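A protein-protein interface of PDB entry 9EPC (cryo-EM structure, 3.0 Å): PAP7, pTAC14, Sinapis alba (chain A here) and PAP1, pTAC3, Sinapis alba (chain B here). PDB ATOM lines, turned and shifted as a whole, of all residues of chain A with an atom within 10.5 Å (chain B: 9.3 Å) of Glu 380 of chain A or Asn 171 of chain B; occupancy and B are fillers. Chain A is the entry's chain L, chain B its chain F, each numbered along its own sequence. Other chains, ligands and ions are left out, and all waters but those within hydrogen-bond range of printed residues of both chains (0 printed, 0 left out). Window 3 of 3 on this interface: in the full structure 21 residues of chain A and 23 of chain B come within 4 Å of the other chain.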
ATOM      1  N   SER A 364     -11.246   0.817  23.087  1.00  0.00           N
ATOM      2  CA  SER A 364     -11.479  -0.612  23.257  1.00  0.00           C
ATOM      3  C   SER A 364     -12.727  -0.896  24.077  1.00  0.00           C
ATOM      4  O   SER A 364     -13.428  -1.878  23.810  1.00  0.00           O
ATOM      5  CB  SER A 364     -10.265  -1.264  23.913  1.00  0.00           C
ATOM      6  OG  SER A 364     -10.052  -0.734  25.208  1.00  0.00           O
ATOM      7  N   PHE A 366     -15.514   0.430  24.071  1.00  0.00           N
ATOM      8  CA  PHE A 366     -16.697   0.465  23.221  1.00  0.00           C
ATOM      9  C   PHE A 366     -16.501  -0.319  21.930  1.00  0.00           C
ATOM     10  O   PHE A 366     -17.265  -0.137  20.977  1.00  0.00           O
ATOM     11  CB  PHE A 366     -17.089   1.910  22.914  1.00  0.00           C
ATOM     12  CG  PHE A 366     -17.465   2.701  24.129  1.00  0.00           C
ATOM     13  CD1 PHE A 366     -18.628   2.418  24.821  1.00  0.00           C
ATOM     14  CD2 PHE A 366     -16.656   3.729  24.579  1.00  0.00           C
ATOM     15  CE1 PHE A 366     -18.978   3.143  25.942  1.00  0.00           C
ATOM     16  CE2 PHE A 366     -17.001   4.458  25.699  1.00  0.00           C
ATOM     17  CZ  PHE A 366     -18.163   4.165  26.380  1.00  0.00           C
ATOM     18  N   ASN A 367     -15.489  -1.188  21.884  1.00  0.00           N
ATOM     19  CA  ASN A 367     -15.216  -2.032  20.720  1.00  0.00           C
ATOM     20  C   ASN A 367     -15.023  -1.199  19.456  1.00  0.00           C
ATOM     21  O   ASN A 367     -15.537  -1.529  18.386  1.00  0.00           O
ATOM     22  CB  ASN A 367     -16.319  -3.073  20.524  1.00  0.00           C
ATOM     23  CG  ASN A 367     -16.463  -3.995  21.715  1.00  0.00           C
ATOM     24  OD1 ASN A 367     -17.485  -3.991  22.398  1.00  0.00           O
ATOM     25  ND2 ASN A 367     -15.433  -4.793  21.972  1.00  0.00           N
ATOM     26  N   ILE A 368     -14.279  -0.105  19.582  1.00  0.00           N
ATOM     27  CA  ILE A 368     -13.928   0.747  18.452  1.00  0.00           C
ATOM     28  C   ILE A 368     -12.502   0.418  18.039  1.00  0.00           C
ATOM     29  O   ILE A 368     -11.587   0.433  18.871  1.00  0.00           O
ATOM     30  CB  ILE A 368     -14.073   2.236  18.805  1.00  0.00           C
ATOM     31  CG1 ILE A 368     -15.495   2.534  19.279  1.00  0.00           C
ATOM     32  CG2 ILE A 368     -13.720   3.100  17.608  1.00  0.00           C
ATOM     33  CD1 ILE A 368     -15.737   3.993  19.598  1.00  0.00           C
ATOM     34  N   PHE A 369     -12.310   0.119  16.757  1.00  0.00           N
ATOM     35  CA  PHE A 369     -11.021  -0.319  16.245  1.00  0.00           C
ATOM     36  C   PHE A 369     -10.670   0.479  14.996  1.00  0.00           C
ATOM     37  O   PHE A 369     -11.461   1.290  14.503  1.00  0.00           O
ATOM     38  CB  PHE A 369     -11.033  -1.822  15.944  1.00  0.00           C
ATOM     39  CG  PHE A 369     -11.561  -2.658  17.070  1.00  0.00           C
ATOM     40  CD1 PHE A 369     -10.736  -3.035  18.115  1.00  0.00           C
ATOM     41  CD2 PHE A 369     -12.883  -3.065  17.087  1.00  0.00           C
ATOM     42  CE1 PHE A 369     -11.219  -3.803  19.154  1.00  0.00           C
ATOM     43  CE2 PHE A 369     -13.373  -3.834  18.122  1.00  0.00           C
ATOM     44  CZ  PHE A 369     -12.540  -4.204  19.158  1.00  0.00           C
ATOM     45  N   TYR A 376     -14.564   2.690  13.636  1.00  0.00           N
ATOM     46  CA  TYR A 376     -15.831   1.991  13.489  1.00  0.00           C
ATOM     47  C   TYR A 376     -16.019   1.070  14.684  1.00  0.00           C
ATOM     48  O   TYR A 376     -15.062   0.727  15.383  1.00  0.00           O
ATOM     49  CB  TYR A 376     -15.893   1.199  12.180  1.00  0.00           C
ATOM     50  CG  TYR A 376     -15.063  -0.061  12.187  1.00  0.00           C
ATOM     51  CD1 TYR A 376     -13.688  -0.009  12.011  1.00  0.00           C
ATOM     52  CD2 TYR A 376     -15.656  -1.304  12.361  1.00  0.00           C
ATOM     53  CE1 TYR A 376     -12.925  -1.160  12.014  1.00  0.00           C
ATOM     54  CE2 TYR A 376     -14.903  -2.458  12.366  1.00  0.00           C
ATOM     55  CZ  TYR A 376     -13.538  -2.382  12.191  1.00  0.00           C
ATOM     56  OH  TYR A 376     -12.785  -3.533  12.196  1.00  0.00           O
ATOM     57  N   HIS A 377     -17.266   0.667  14.900  1.00  0.00           N
ATOM     58  CA  HIS A 377     -17.641  -0.172  16.027  1.00  0.00           C
ATOM     59  C   HIS A 377     -17.947  -1.585  15.554  1.00  0.00           C
ATOM     60  O   HIS A 377     -18.543  -1.780  14.490  1.00  0.00           O
ATOM     61  CB  HIS A 377     -18.855   0.404  16.759  1.00  0.00           C
ATOM     62  CG  HIS A 377     -19.581  -0.598  17.600  1.00  0.00           C
ATOM     63  ND1 HIS A 377     -20.801  -1.126  17.238  1.00  0.00           N
ATOM     64  CD2 HIS A 377     -19.254  -1.179  18.778  1.00  0.00           C
ATOM     65  CE1 HIS A 377     -21.199  -1.983  18.161  1.00  0.00           C
ATOM     66  NE2 HIS A 377     -20.277  -2.035  19.106  1.00  0.00           N
ATOM     67  N   ASP A 378     -17.533  -2.568  16.349  1.00  0.00           N
ATOM     68  CA  ASP A 378     -17.810  -3.967  16.063  1.00  0.00           C
ATOM     69  C   ASP A 378     -19.065  -4.395  16.813  1.00  0.00           C
ATOM     70  O   ASP A 378     -19.160  -4.216  18.031  1.00  0.00           O
ATOM     71  CB  ASP A 378     -16.620  -4.843  16.457  1.00  0.00           C
ATOM     72  CG  ASP A 378     -16.745  -6.267  15.950  1.00  0.00           C
ATOM     73  OD1 ASP A 378     -17.780  -6.913  16.213  1.00  0.00           O
ATOM     74  OD2 ASP A 378     -15.803  -6.743  15.283  1.00  0.00           O
ATOM     75  N   SER A 379     -20.021  -4.969  16.082  1.00  0.00           N
ATOM     76  CA  SER A 379     -21.310  -5.308  16.674  1.00  0.00           C
ATOM     77  C   SER A 379     -21.256  -6.625  17.437  1.00  0.00           C
ATOM     78  O   SER A 379     -21.675  -6.694  18.599  1.00  0.00           O
ATOM     79  CB  SER A 379     -22.383  -5.367  15.585  1.00  0.00           C
ATOM     80  OG  SER A 379     -22.065  -6.350  14.615  1.00  0.00           O
ATOM     81  N   GLU A 380     -20.744  -7.684  16.802  1.00  0.00           N
ATOM     82  CA  GLU A 380     -20.775  -9.003  17.426  1.00  0.00           C
ATOM     83  C   GLU A 380     -19.890  -9.069  18.665  1.00  0.00           C
ATOM     84  O   GLU A 380     -20.214  -9.792  19.614  1.00  0.00           O
ATOM     85  CB  GLU A 380     -20.366 -10.080  16.421  1.00  0.00           C
ATOM     86  CG  GLU A 380     -19.036  -9.839  15.725  1.00  0.00           C
ATOM     87  CD  GLU A 380     -19.169  -8.957  14.498  1.00  0.00           C
ATOM     88  OE1 GLU A 380     -20.306  -8.552  14.176  1.00  0.00           O
ATOM     89  OE2 GLU A 380     -18.137  -8.669  13.858  1.00  0.00           O
ATOM     90  N   LEU A 381     -18.774  -8.337  18.676  1.00  0.00           N
ATOM     91  CA  LEU A 381     -17.920  -8.319  19.860  1.00  0.00           C
ATOM     92  C   LEU A 381     -18.651  -7.725  21.057  1.00  0.00           C
ATOM     93  O   LEU A 381     -18.557  -8.248  22.174  1.00  0.00           O
ATOM     94  CB  LEU A 381     -16.641  -7.538  19.574  1.00  0.00           C
ATOM     95  CG  LEU A 381     -15.652  -8.214  18.627  1.00  0.00           C
ATOM     96  CD1 LEU A 381     -14.464  -7.305  18.368  1.00  0.00           C
ATOM     97  CD2 LEU A 381     -15.201  -9.547  19.204  1.00  0.00           C
ATOM     98  N   SER A 382     -19.386  -6.634  20.843  1.00  0.00           N
ATOM     99  CA  SER A 382     -20.127  -6.008  21.928  1.00  0.00           C
ATOM    100  C   SER A 382     -21.364  -6.804  22.320  1.00  0.00           C
ATOM    101  O   SER A 382     -21.891  -6.607  23.420  1.00  0.00           O
ATOM    102  CB  SER A 382     -20.520  -4.587  21.529  1.00  0.00           C
ATOM    103  OG  SER A 382     -21.331  -4.592  20.366  1.00  0.00           O
ATOM    104  N   GLY A 383     -21.835  -7.692  21.450  1.00  0.00           N
ATOM    105  CA  GLY A 383     -23.003  -8.507  21.724  1.00  0.00           C
ATOM    106  C   GLY A 383     -24.306  -7.789  21.443  1.00  0.00           C
ATOM    107  O   GLY A 383     -24.942  -8.035  20.413  1.00  0.00           O
ATOM    108  N   ASP A 384     -24.725  -6.905  22.350  1.00  0.00           N
ATOM    109  CA  ASP A 384     -25.851  -6.015  22.084  1.00  0.00           C
ATOM    110  C   ASP A 384     -25.441  -4.551  22.144  1.00  0.00           C
ATOM    111  O   ASP A 384     -25.530  -3.854  21.129  1.00  0.00           O
ATOM    112  CB  ASP A 384     -26.992  -6.308  23.067  1.00  0.00           C
ATOM    113  CG  ASP A 384     -26.522  -6.363  24.507  1.00  0.00           C
ATOM    114  OD1 ASP A 384     -25.341  -6.696  24.737  1.00  0.00           O
ATOM    115  OD2 ASP A 384     -27.334  -6.069  25.410  1.00  0.00           O
ATOM    116  N   ASP A 385     -24.961  -4.083  23.297  1.00  0.00           N
ATOM    117  CA  ASP A 385     -24.419  -2.737  23.490  1.00  0.00           C
ATOM    118  C   ASP A 385     -25.247  -1.677  22.765  1.00  0.00           C
ATOM    119  O   ASP A 385     -24.783  -0.997  21.850  1.00  0.00           O
ATOM    120  CB  ASP A 385     -22.956  -2.676  23.059  1.00  0.00           C
ATOM    121  CG  ASP A 385     -22.193  -1.567  23.752  1.00  0.00           C
ATOM    122  OD1 ASP A 385     -22.817  -0.800  24.516  1.00  0.00           O
ATOM    123  OD2 ASP A 385     -20.967  -1.461  23.533  1.00  0.00           O
ATOM    124  N   VAL A 388     -23.710   2.114  22.262  1.00  0.00           N
ATOM    125  CA  VAL A 388     -22.697   2.553  21.309  1.00  0.00           C
ATOM    126  C   VAL A 388     -23.334   2.796  19.947  1.00  0.00           C
ATOM    127  O   VAL A 388     -24.157   2.001  19.472  1.00  0.00           O
ATOM    128  CB  VAL A 388     -21.552   1.530  21.224  1.00  0.00           C
ATOM    129  CG1 VAL A 388     -22.065   0.172  20.786  1.00  0.00           C
ATOM    130  CG2 VAL A 388     -20.467   2.020  20.277  1.00  0.00           C
ATOM    131  N   ARG B 138     -11.335 -12.907  27.748  1.00  0.00           N
ATOM    132  CA  ARG B 138     -10.754 -12.430  26.500  1.00  0.00           C
ATOM    133  C   ARG B 138      -9.771 -11.297  26.775  1.00  0.00           C
ATOM    134  O   ARG B 138     -10.133 -10.314  27.430  1.00  0.00           O
ATOM    135  CB  ARG B 138     -11.855 -11.959  25.553  1.00  0.00           C
ATOM    136  CG  ARG B 138     -12.957 -12.985  25.343  1.00  0.00           C
ATOM    137  CD  ARG B 138     -14.063 -12.459  24.442  1.00  0.00           C
ATOM    138  NE  ARG B 138     -13.647 -12.365  23.047  1.00  0.00           N
ATOM    139  CZ  ARG B 138     -13.245 -11.248  22.457  1.00  0.00           C
ATOM    140  NH1 ARG B 138     -13.187 -10.102  23.114  1.00  0.00           N
ATOM    141  NH2 ARG B 138     -12.897 -11.281  21.174  1.00  0.00           N
ATOM    142  N   PRO B 139      -8.529 -11.400  26.307  1.00  0.00           N
ATOM    143  CA  PRO B 139      -7.570 -10.309  26.513  1.00  0.00           C
ATOM    144  C   PRO B 139      -7.995  -9.043  25.789  1.00  0.00           C
ATOM    145  O   PRO B 139      -8.631  -9.082  24.734  1.00  0.00           O
ATOM    146  CB  PRO B 139      -6.265 -10.867  25.931  1.00  0.00           C
ATOM    147  CG  PRO B 139      -6.459 -12.349  25.894  1.00  0.00           C
ATOM    148  CD  PRO B 139      -7.915 -12.559  25.642  1.00  0.00           C
ATOM    149  N   PRO B 141      -7.667  -5.718  23.509  1.00  0.00           N
ATOM    150  CA  PRO B 141      -6.888  -5.437  22.291  1.00  0.00           C
ATOM    151  C   PRO B 141      -5.614  -4.658  22.554  1.00  0.00           C
ATOM    152  O   PRO B 141      -4.614  -4.880  21.860  1.00  0.00           O
ATOM    153  CB  PRO B 141      -7.872  -4.639  21.426  1.00  0.00           C
ATOM    154  CG  PRO B 141      -9.219  -5.052  21.914  1.00  0.00           C
ATOM    155  CD  PRO B 141      -9.063  -5.266  23.389  1.00  0.00           C
ATOM    156  N   MET B 144      -3.113  -7.092  23.357  1.00  0.00           N
ATOM    157  CA  MET B 144      -2.721  -7.805  22.149  1.00  0.00           C
ATOM    158  C   MET B 144      -1.814  -6.951  21.272  1.00  0.00           C
ATOM    159  O   MET B 144      -0.827  -7.448  20.719  1.00  0.00           O
ATOM    160  CB  MET B 144      -3.967  -8.236  21.381  1.00  0.00           C
ATOM    161  CG  MET B 144      -4.946  -9.033  22.216  1.00  0.00           C
ATOM    162  SD  MET B 144      -4.220 -10.568  22.809  1.00  0.00           S
ATOM    163  CE  MET B 144      -3.880 -11.385  21.256  1.00  0.00           C
ATOM    164  N   LEU B 163       0.624 -14.444  17.313  1.00  0.00           N
ATOM    165  CA  LEU B 163      -0.272 -13.578  18.071  1.00  0.00           C
ATOM    166  C   LEU B 163      -1.336 -12.957  17.174  1.00  0.00           C
ATOM    167  O   LEU B 163      -2.498 -12.831  17.579  1.00  0.00           O
ATOM    168  CB  LEU B 163       0.532 -12.492  18.781  1.00  0.00           C
ATOM    169  CG  LEU B 163       1.566 -13.002  19.784  1.00  0.00           C
ATOM    170  CD1 LEU B 163       2.434 -11.862  20.283  1.00  0.00           C
ATOM    171  CD2 LEU B 163       0.878 -13.704  20.941  1.00  0.00           C
ATOM    172  N   LEU B 164      -0.958 -12.555  15.959  1.00  0.00           N
ATOM    173  CA  LEU B 164      -1.938 -11.998  15.033  1.00  0.00           C
ATOM    174  C   LEU B 164      -2.998 -13.028  14.672  1.00  0.00           C
ATOM    175  O   LEU B 164      -4.183 -12.694  14.546  1.00  0.00           O
ATOM    176  CB  LEU B 164      -1.244 -11.480  13.774  1.00  0.00           C
ATOM    177  CG  LEU B 164      -0.415 -10.205  13.931  1.00  0.00           C
ATOM    178  CD1 LEU B 164       0.156  -9.772  12.591  1.00  0.00           C
ATOM    179  CD2 LEU B 164      -1.254  -9.097  14.541  1.00  0.00           C
ATOM    180  N   ALA B 165      -2.591 -14.287  14.498  1.00  0.00           N
ATOM    181  CA  ALA B 165      -3.561 -15.345  14.242  1.00  0.00           C
ATOM    182  C   ALA B 165      -4.520 -15.500  15.414  1.00  0.00           C
ATOM    183  O   ALA B 165      -5.702 -15.807  15.224  1.00  0.00           O
ATOM    184  CB  ALA B 165      -2.840 -16.662  13.956  1.00  0.00           C
ATOM    185  N   ALA B 166      -4.026 -15.291  16.635  1.00  0.00           N
ATOM    186  CA  ALA B 166      -4.897 -15.352  17.804  1.00  0.00           C
ATOM    187  C   ALA B 166      -5.955 -14.259  17.758  1.00  0.00           C
ATOM    188  O   ALA B 166      -7.119 -14.499  18.101  1.00  0.00           O
ATOM    189  CB  ALA B 166      -4.069 -15.249  19.083  1.00  0.00           C
ATOM    190  N   MET B 167      -5.573 -13.049  17.337  1.00  0.00           N
ATOM    191  CA  MET B 167      -6.542 -11.960  17.255  1.00  0.00           C
ATOM    192  C   MET B 167      -7.658 -12.288  16.273  1.00  0.00           C
ATOM    193  O   MET B 167      -8.838 -12.051  16.560  1.00  0.00           O
ATOM    194  CB  MET B 167      -5.851 -10.661  16.848  1.00  0.00           C
ATOM    195  CG  MET B 167      -4.730 -10.222  17.767  1.00  0.00           C
ATOM    196  SD  MET B 167      -4.665  -8.428  17.929  1.00  0.00           S
ATOM    197  CE  MET B 167      -5.336  -7.915  16.352  1.00  0.00           C
ATOM    198  N   GLU B 168      -7.306 -12.828  15.105  1.00  0.00           N
ATOM    199  CA  GLU B 168      -8.326 -13.259  14.157  1.00  0.00           C
ATOM    200  C   GLU B 168      -9.165 -14.386  14.743  1.00  0.00           C
ATOM    201  O   GLU B 168     -10.391 -14.411  14.576  1.00  0.00           O
ATOM    202  CB  GLU B 168      -7.672 -13.691  12.845  1.00  0.00           C
ATOM    203  CG  GLU B 168      -8.653 -13.962  11.716  1.00  0.00           C
ATOM    204  CD  GLU B 168      -7.955 -14.244  10.400  1.00  0.00           C
ATOM    205  OE1 GLU B 168      -6.707 -14.199  10.367  1.00  0.00           O
ATOM    206  OE2 GLU B 168      -8.652 -14.506   9.397  1.00  0.00           O
ATOM    207  N   LYS B 169      -8.520 -15.329  15.434  1.00  0.00           N
ATOM    208  CA  LYS B 169      -9.265 -16.345  16.166  1.00  0.00           C
ATOM    209  C   LYS B 169     -10.067 -15.725  17.301  1.00  0.00           C
ATOM    210  O   LYS B 169     -11.128 -16.243  17.669  1.00  0.00           O
ATOM    211  CB  LYS B 169      -8.304 -17.412  16.697  1.00  0.00           C
ATOM    212  CG  LYS B 169      -8.985 -18.619  17.315  1.00  0.00           C
ATOM    213  CD  LYS B 169      -8.035 -19.806  17.389  1.00  0.00           C
ATOM    214  CE  LYS B 169      -6.768 -19.460  18.156  1.00  0.00           C
ATOM    215  NZ  LYS B 169      -5.824 -20.613  18.216  1.00  0.00           N
ATOM    216  N   LEU B 170      -9.584 -14.617  17.860  1.00  0.00           N
ATOM    217  CA  LEU B 170     -10.336 -13.850  18.843  1.00  0.00           C
ATOM    218  C   LEU B 170     -11.301 -12.866  18.196  1.00  0.00           C
ATOM    219  O   LEU B 170     -12.040 -12.183  18.913  1.00  0.00           O
ATOM    220  CB  LEU B 170      -9.370 -13.106  19.771  1.00  0.00           C
ATOM    221  CG  LEU B 170      -9.883 -12.683  21.147  1.00  0.00           C
ATOM    222  CD1 LEU B 170     -10.552 -13.853  21.845  1.00  0.00           C
ATOM    223  CD2 LEU B 170      -8.743 -12.140  21.988  1.00  0.00           C
ATOM    224  N   ASN B 171     -11.306 -12.783  16.864  1.00  0.00           N
ATOM    225  CA  ASN B 171     -12.219 -11.927  16.109  1.00  0.00           C
ATOM    226  C   ASN B 171     -12.018 -10.452  16.467  1.00  0.00           C
ATOM    227  O   ASN B 171     -12.914  -9.771  16.964  1.00  0.00           O
ATOM    228  CB  ASN B 171     -13.674 -12.363  16.322  1.00  0.00           C
ATOM    229  CG  ASN B 171     -14.636 -11.680  15.371  1.00  0.00           C
ATOM    230  OD1 ASN B 171     -15.271 -10.685  15.719  1.00  0.00           O
ATOM    231  ND2 ASN B 171     -14.749 -12.215  14.161  1.00  0.00           N
ATOM    232  N   TYR B 172     -10.807  -9.970  16.206  1.00  0.00           N
ATOM    233  CA  TYR B 172     -10.444  -8.573  16.408  1.00  0.00           C
ATOM    234  C   TYR B 172      -9.996  -7.960  15.084  1.00  0.00           C
ATOM    235  O   TYR B 172     -10.019  -8.605  14.033  1.00  0.00           O
ATOM    236  CB  TYR B 172      -9.349  -8.439  17.470  1.00  0.00           C
ATOM    237  CG  TYR B 172      -9.861  -8.505  18.890  1.00  0.00           C
ATOM    238  CD1 TYR B 172     -11.208  -8.332  19.169  1.00  0.00           C
ATOM    239  CD2 TYR B 172      -8.995  -8.730  19.951  1.00  0.00           C
ATOM    240  CE1 TYR B 172     -11.681  -8.388  20.464  1.00  0.00           C
ATOM    241  CE2 TYR B 172      -9.459  -8.786  21.249  1.00  0.00           C
ATOM    242  CZ  TYR B 172     -10.803  -8.616  21.499  1.00  0.00           C
ATOM    243  OH  TYR B 172     -11.270  -8.672  22.792  1.00  0.00           O
ATOM    244  N   ASP B 173      -9.583  -6.695  15.144  1.00  0.00           N
ATOM    245  CA  ASP B 173      -9.100  -5.971  13.968  1.00  0.00           C
ATOM    246  C   ASP B 173      -7.610  -6.254  13.827  1.00  0.00           C
ATOM    247  O   ASP B 173      -6.766  -5.566  14.403  1.00  0.00           O
ATOM    248  CB  ASP B 173      -9.383  -4.480  14.094  1.00  0.00           C
ATOM    249  CG  ASP B 173      -9.212  -3.735  12.780  1.00  0.00           C
ATOM    250  OD1 ASP B 173      -8.488  -4.233  11.892  1.00  0.00           O
ATOM    251  OD2 ASP B 173      -9.804  -2.645  12.635  1.00  0.00           O
ATOM    252  N   ILE B 174      -7.286  -7.282  13.041  1.00  0.00           N
ATOM    253  CA  ILE B 174      -5.892  -7.674  12.865  1.00  0.00           C
ATOM    254  C   ILE B 174      -5.124  -6.619  12.083  1.00  0.00           C
ATOM    255  O   ILE B 174      -3.908  -6.474  12.255  1.00  0.00           O
ATOM    256  CB  ILE B 174      -5.803  -9.051  12.183  1.00  0.00           C
ATOM    257  CG1 ILE B 174      -6.828 -10.018  12.779  1.00  0.00           C
ATOM    258  CG2 ILE B 174      -4.402  -9.626  12.320  1.00  0.00           C
ATOM    259  CD1 ILE B 174      -8.073 -10.194  11.930  1.00  0.00           C
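Among the printed residues, merely in contact across the chains: Leu 381 of chain A with Asn 171 of chain B, Leu 381 of chain A with Arg 138 of chain B, Leu 381 of chain A with Tyr 172 of chain B, Phe 369 of chain A with Asp 173 of chain B, Phe 369 of chain A with Pro 141 of chain B and Glu 380 of chain A with Asn 171 of chain B.
N of Tyr 172 of chain B sits at hydrogen-bond distance from O of Met 167 of chain B (2.9 Å). The backbone carbonyl oxygen (O) of Leu 170 of chain B lies within hydrogen-bond range of the guanidinium group (NH2) of Arg 138 of chain B. O of Pro 139 of chain B is in hydrogen-bond range of OH of Tyr 172 of chain B (3.3 Å). The guanidinium group (NH1) of Arg 138 of chain B sits at hydrogen-bond distance from the side-chain hydroxyl (OH) of Tyr 172 of chain B, at 2.4 Å. The backbone NH (N) of Phe 369 of chain A is in hydrogen-bond range of the backbone carbonyl oxygen (O) of Tyr 376 of chain A, at 3.1 Å. N of Glu 380 of chain A sits close to OD1 of Asp 378 of chain A, at 3.1 Å.
Hydrophobic or aromatic side chains of chain A that line the printed part of chain B: Phe 369, Tyr 376 and Leu 381. Hydrophobic or aromatic side chains of chain B that line the printed part of chain A: Pro 141 and Tyr 172. Among the printed residues, 7 pairs touch across the chains. Among the printed residues, no Asp or Glu carboxylate lies within 4 Å of a Lys or Arg side-chain nitrogen of the other chain.
Of chain B, only Asn 171 comes within 4 Å of Glu 380 of chain A. Of the printed residues of chain B, Leu 381 of chain A touches Arg 138 (3.5 Å), Asn 171 (3.2 Å) and Tyr 172 (3.5 Å). No residue of chain B comes within 4 Å of Gly 383 of chain A. No residue of chain A comes within 4 Å of Leu 170 of chain B. Of chain A, only Leu 381 comes within 4 Å of Tyr 172 of chain B. Printed residues of chain A within 4 Å of Asp 173 of chain B: Phe 369 and Tyr 376. Printed residues of chain B within 4 Å of Phe 369 of chain A: Pro 141 and Asp 173. The nearest printed residue of chain A that does not touch Asn 171 of chain B is Asp 378 of chain A (4.002 Å). The nearest printed residue of chain B that does not touch Tyr 376 of chain A is Tyr 172 of chain B (6.0 Å).
The side-chain carboxylate (OD2) of Asp 173 of chain B sits at hydrogen-bond distance from the side-chain hydroxyl (OH) of Tyr 376 of chain A.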
